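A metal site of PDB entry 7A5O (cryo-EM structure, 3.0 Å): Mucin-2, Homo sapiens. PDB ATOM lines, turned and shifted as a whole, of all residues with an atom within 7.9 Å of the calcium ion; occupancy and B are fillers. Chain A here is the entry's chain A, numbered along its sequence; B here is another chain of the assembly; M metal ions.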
ATOM      1  N   THR A 381     -36.466 -15.554 -20.695  1.00  0.00           N
ATOM      2  CA  THR A 381     -35.198 -14.972 -21.099  1.00  0.00           C
ATOM      3  C   THR A 381     -35.007 -15.126 -22.603  1.00  0.00           C
ATOM      4  O   THR A 381     -35.866 -15.656 -23.304  1.00  0.00           O
ATOM      5  CB  THR A 381     -34.044 -15.610 -20.330  1.00  0.00           C
ATOM      6  OG1 THR A 381     -33.948 -16.987 -20.697  1.00  0.00           O
ATOM      7  CG2 THR A 381     -34.281 -15.544 -18.847  1.00  0.00           C
ATOM      8  N   PHE A 382     -33.855 -14.681 -23.104  1.00  0.00           N
ATOM      9  CA  PHE A 382     -33.579 -14.837 -24.522  1.00  0.00           C
ATOM     10  C   PHE A 382     -33.321 -16.277 -24.927  1.00  0.00           C
ATOM     11  O   PHE A 382     -33.348 -16.572 -26.132  1.00  0.00           O
ATOM     12  CB  PHE A 382     -32.374 -14.013 -24.945  1.00  0.00           C
ATOM     13  CG  PHE A 382     -32.566 -12.529 -24.923  1.00  0.00           C
ATOM     14  CD1 PHE A 382     -33.280 -11.904 -25.927  1.00  0.00           C
ATOM     15  CD2 PHE A 382     -31.932 -11.748 -23.987  1.00  0.00           C
ATOM     16  CE1 PHE A 382     -33.433 -10.539 -25.932  1.00  0.00           C
ATOM     17  CE2 PHE A 382     -32.080 -10.377 -23.997  1.00  0.00           C
ATOM     18  CZ  PHE A 382     -32.837  -9.782 -24.970  1.00  0.00           C
ATOM     19  N   ASP A 383     -33.050 -17.169 -23.990  1.00  0.00           N
ATOM     20  CA  ASP A 383     -32.646 -18.546 -24.264  1.00  0.00           C
ATOM     21  C   ASP A 383     -33.636 -19.544 -23.696  1.00  0.00           C
ATOM     22  O   ASP A 383     -33.242 -20.599 -23.200  1.00  0.00           O
ATOM     23  CB  ASP A 383     -31.256 -18.824 -23.698  1.00  0.00           C
ATOM     24  CG  ASP A 383     -30.178 -18.080 -24.424  1.00  0.00           C
ATOM     25  OD1 ASP A 383     -30.365 -17.807 -25.621  1.00  0.00           O
ATOM     26  OD2 ASP A 383     -29.141 -17.779 -23.813  1.00  0.00           O
ATOM     27  N   LYS A 385     -36.092 -20.516 -20.738  1.00  0.00           N
ATOM     28  CA  LYS A 385     -35.875 -20.270 -19.300  1.00  0.00           C
ATOM     29  C   LYS A 385     -36.926 -19.309 -18.735  1.00  0.00           C
ATOM     30  O   LYS A 385     -36.685 -18.118 -18.540  1.00  0.00           O
ATOM     31  CB  LYS A 385     -34.434 -19.788 -19.084  1.00  0.00           C
ATOM     32  CG  LYS A 385     -33.986 -19.634 -17.630  1.00  0.00           C
ATOM     33  CD  LYS A 385     -33.809 -20.974 -16.989  1.00  0.00           C
ATOM     34  CE  LYS A 385     -33.204 -20.840 -15.621  1.00  0.00           C
ATOM     35  NZ  LYS A 385     -33.053 -22.170 -14.995  1.00  0.00           N
ATOM     36  N   GLY A 502     -24.329 -12.989 -26.482  1.00  0.00           N
ATOM     37  CA  GLY A 502     -23.334 -13.021 -25.431  1.00  0.00           C
ATOM     38  C   GLY A 502     -22.849 -11.665 -24.991  1.00  0.00           C
ATOM     39  O   GLY A 502     -21.767 -11.569 -24.411  1.00  0.00           O
ATOM     40  N   CYS A 508     -32.937 -10.637 -18.363  1.00  0.00           N
ATOM     41  CA  CYS A 508     -33.206 -11.394 -19.566  1.00  0.00           C
ATOM     42  C   CYS A 508     -32.082 -12.362 -19.914  1.00  0.00           C
ATOM     43  O   CYS A 508     -32.140 -12.979 -20.974  1.00  0.00           O
ATOM     44  CB  CYS A 508     -33.452 -10.451 -20.734  1.00  0.00           C
ATOM     45  SG  CYS A 508     -34.987  -9.522 -20.671  1.00  0.00           S
ATOM     46  N   GLY A 509     -31.081 -12.503 -19.063  1.00  0.00           N
ATOM     47  CA  GLY A 509     -30.009 -13.442 -19.319  1.00  0.00           C
ATOM     48  C   GLY A 509     -28.928 -12.835 -20.187  1.00  0.00           C
ATOM     49  O   GLY A 509     -28.872 -11.634 -20.414  1.00  0.00           O
ATOM     50  N   ASN A 510     -28.049 -13.703 -20.669  1.00  0.00           N
ATOM     51  CA  ASN A 510     -26.923 -13.251 -21.470  1.00  0.00           C
ATOM     52  C   ASN A 510     -26.969 -13.654 -22.936  1.00  0.00           C
ATOM     53  O   ASN A 510     -26.129 -13.159 -23.701  1.00  0.00           O
ATOM     54  CB  ASN A 510     -25.589 -13.699 -20.847  1.00  0.00           C
ATOM     55  CG  ASN A 510     -25.487 -15.184 -20.665  1.00  0.00           C
ATOM     56  OD1 ASN A 510     -26.369 -15.943 -21.026  1.00  0.00           O
ATOM     57  ND2 ASN A 510     -24.374 -15.613 -20.080  1.00  0.00           N
ATOM     58  N   PHE A 511     -27.905 -14.527 -23.341  1.00  0.00           N
ATOM     59  CA  PHE A 511     -28.181 -14.858 -24.753  1.00  0.00           C
ATOM     60  C   PHE A 511     -26.934 -15.438 -25.428  1.00  0.00           C
ATOM     61  O   PHE A 511     -26.244 -14.790 -26.202  1.00  0.00           O
ATOM     62  CB  PHE A 511     -28.769 -13.611 -25.445  1.00  0.00           C
ATOM     63  CG  PHE A 511     -29.080 -13.775 -26.918  1.00  0.00           C
ATOM     64  CD1 PHE A 511     -29.959 -14.734 -27.366  1.00  0.00           C
ATOM     65  CD2 PHE A 511     -28.659 -12.810 -27.818  1.00  0.00           C
ATOM     66  CE1 PHE A 511     -30.290 -14.829 -28.704  1.00  0.00           C
ATOM     67  CE2 PHE A 511     -28.998 -12.890 -29.145  1.00  0.00           C
ATOM     68  CZ  PHE A 511     -29.816 -13.900 -29.591  1.00  0.00           C
ATOM     69  N   ASN A 512     -26.607 -16.663 -24.999  1.00  0.00           N
ATOM     70  CA  ASN A 512     -25.458 -17.393 -25.524  1.00  0.00           C
ATOM     71  C   ASN A 512     -25.765 -18.814 -25.989  1.00  0.00           C
ATOM     72  O   ASN A 512     -24.844 -19.536 -26.365  1.00  0.00           O
ATOM     73  CB  ASN A 512     -24.323 -17.420 -24.493  1.00  0.00           C
ATOM     74  CG  ASN A 512     -24.715 -18.070 -23.167  1.00  0.00           C
ATOM     75  OD1 ASN A 512     -25.840 -18.537 -22.981  1.00  0.00           O
ATOM     76  ND2 ASN A 512     -23.772 -18.126 -22.256  1.00  0.00           N
ATOM     77  N   GLY A 513     -27.029 -19.243 -25.960  1.00  0.00           N
ATOM     78  CA  GLY A 513     -27.414 -20.562 -26.401  1.00  0.00           C
ATOM     79  C   GLY A 513     -27.732 -21.530 -25.285  1.00  0.00           C
ATOM     80  O   GLY A 513     -28.646 -22.339 -25.422  1.00  0.00           O
ATOM     81  N   LEU A 514     -26.989 -21.473 -24.184  1.00  0.00           N
ATOM     82  CA  LEU A 514     -27.246 -22.276 -22.996  1.00  0.00           C
ATOM     83  C   LEU A 514     -28.216 -21.535 -22.085  1.00  0.00           C
ATOM     84  O   LEU A 514     -28.149 -20.316 -21.963  1.00  0.00           O
ATOM     85  CB  LEU A 514     -25.937 -22.549 -22.264  1.00  0.00           C
ATOM     86  CG  LEU A 514     -25.864 -23.370 -20.980  1.00  0.00           C
ATOM     87  CD1 LEU A 514     -26.229 -24.810 -21.189  1.00  0.00           C
ATOM     88  CD2 LEU A 514     -24.464 -23.250 -20.434  1.00  0.00           C
ATOM     89  N   GLU A 515     -29.113 -22.266 -21.437  1.00  0.00           N
ATOM     90  CA  GLU A 515     -30.018 -21.653 -20.463  1.00  0.00           C
ATOM     91  C   GLU A 515     -29.699 -22.090 -19.044  1.00  0.00           C
ATOM     92  O   GLU A 515     -30.442 -21.754 -18.120  1.00  0.00           O
ATOM     93  CB  GLU A 515     -31.480 -21.970 -20.785  1.00  0.00           C
ATOM     94  CG  GLU A 515     -31.866 -23.402 -20.595  1.00  0.00           C
ATOM     95  CD  GLU A 515     -33.306 -23.672 -20.951  1.00  0.00           C
ATOM     96  OE1 GLU A 515     -33.991 -22.731 -21.378  1.00  0.00           O
ATOM     97  OE2 GLU A 515     -33.765 -24.818 -20.794  1.00  0.00           O
ATOM     98  N   GLY A 516     -28.621 -22.846 -18.849  1.00  0.00           N
ATOM     99  CA  GLY A 516     -28.204 -23.188 -17.497  1.00  0.00           C
ATOM    100  C   GLY A 516     -27.500 -22.048 -16.788  1.00  0.00           C
ATOM    101  O   GLY A 516     -27.487 -22.015 -15.555  1.00  0.00           O
ATOM    102  N   ASP A 517     -26.914 -21.124 -17.546  1.00  0.00           N
ATOM    103  CA  ASP A 517     -26.188 -20.002 -16.968  1.00  0.00           C
ATOM    104  C   ASP A 517     -26.944 -18.686 -17.076  1.00  0.00           C
ATOM    105  O   ASP A 517     -26.321 -17.629 -17.095  1.00  0.00           O
ATOM    106  CB  ASP A 517     -24.802 -19.857 -17.587  1.00  0.00           C
ATOM    107  CG  ASP A 517     -24.842 -19.620 -19.085  1.00  0.00           C
ATOM    108  OD1 ASP A 517     -25.919 -19.681 -19.712  1.00  0.00           O
ATOM    109  OD2 ASP A 517     -23.757 -19.345 -19.654  1.00  0.00           O
ATOM    110  N   ASP A 518     -28.271 -18.717 -17.198  1.00  0.00           N
ATOM    111  CA  ASP A 518     -28.984 -17.455 -17.194  1.00  0.00           C
ATOM    112  C   ASP A 518     -29.098 -16.877 -15.798  1.00  0.00           C
ATOM    113  O   ASP A 518     -29.162 -15.649 -15.650  1.00  0.00           O
ATOM    114  CB  ASP A 518     -30.370 -17.585 -17.832  1.00  0.00           C
ATOM    115  CG  ASP A 518     -30.317 -17.629 -19.348  1.00  0.00           C
ATOM    116  OD1 ASP A 518     -29.397 -17.057 -19.937  1.00  0.00           O
ATOM    117  OD2 ASP A 518     -31.240 -18.200 -19.939  1.00  0.00           O
ATOM    118  N   PHE A 519     -29.085 -17.715 -14.764  1.00  0.00           N
ATOM    119  CA  PHE A 519     -29.092 -17.236 -13.393  1.00  0.00           C
ATOM    120  C   PHE A 519     -27.699 -16.937 -12.864  1.00  0.00           C
ATOM    121  O   PHE A 519     -27.492 -16.934 -11.654  1.00  0.00           O
ATOM    122  CB  PHE A 519     -29.784 -18.224 -12.465  1.00  0.00           C
ATOM    123  CG  PHE A 519     -31.275 -18.307 -12.651  1.00  0.00           C
ATOM    124  CD1 PHE A 519     -31.952 -17.335 -13.369  1.00  0.00           C
ATOM    125  CD2 PHE A 519     -31.987 -19.311 -12.062  1.00  0.00           C
ATOM    126  CE1 PHE A 519     -33.300 -17.414 -13.532  1.00  0.00           C
ATOM    127  CE2 PHE A 519     -33.345 -19.389 -12.215  1.00  0.00           C
ATOM    128  CZ  PHE A 519     -33.997 -18.434 -12.947  1.00  0.00           C
ATOM    129  N   LYS A 520     -26.739 -16.708 -13.748  1.00  0.00           N
ATOM    130  CA  LYS A 520     -25.386 -16.313 -13.371  1.00  0.00           C
ATOM    131  C   LYS A 520     -25.351 -14.832 -13.061  1.00  0.00           C
ATOM    132  O   LYS A 520     -25.620 -13.997 -13.932  1.00  0.00           O
ATOM    133  CB  LYS A 520     -24.434 -16.634 -14.510  1.00  0.00           C
ATOM    134  CG  LYS A 520     -23.005 -16.335 -14.243  1.00  0.00           C
ATOM    135  CD  LYS A 520     -22.194 -16.726 -15.460  1.00  0.00           C
ATOM    136  CE  LYS A 520     -20.742 -16.388 -15.274  1.00  0.00           C
ATOM    137  NZ  LYS A 520     -19.964 -16.753 -16.495  1.00  0.00           N
ATOM    138  N   SER B 979     -27.241 -25.660 -24.905  1.00  0.00           N
ATOM    139  CA  SER B 979     -28.384 -26.559 -24.769  1.00  0.00           C
ATOM    140  C   SER B 979     -29.466 -26.346 -25.805  1.00  0.00           C
ATOM    141  O   SER B 979     -30.508 -27.002 -25.721  1.00  0.00           O
ATOM    142  CB  SER B 979     -29.014 -26.432 -23.397  1.00  0.00           C
ATOM    143  OG  SER B 979     -29.699 -25.207 -23.279  1.00  0.00           O
HETATM  144 CA    CA M   1     -27.452 -18.148 -21.118  1.00  0.00          CA
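The backbone NH (N) of Gly 502 sits close to the backbone carbonyl oxygen (O) of Asn 510, at 3.3 Å. The backbone NH of Asn 512 is in hydrogen-bond range of the side-chain carboxylate of Asp 383, 3.0 Å away. OD2 of Asp 383 is in hydrogen-bond range of N of Gly 513, at 3.3 Å. The backbone NH (N) of Asp 383 sits close to the side-chain hydroxyl (OG1) of Thr 381 (3.4 Å). OD2 of Asp 518 is in hydrogen-bond range of OG1 of Thr 381, 3.1 Å away.
OD2 of Asp 383 touches the calcium ion, 3.2 Å away. Of the 19 residues printed, 6 come within 4 Å of the calcium ion. The nearest printed residue that does not touch the calcium ion is Phe 511 (4.3 Å).
The calcium ion is bound by O of Leu 514 (2.4 Å), OD1 of Asn 510 (2.5 Å), OD1 of Asn 512 (2.5 Å), OD1 of Asp 518 (2.5 Å) and OD1 of Asp 517 (2.6 Å).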
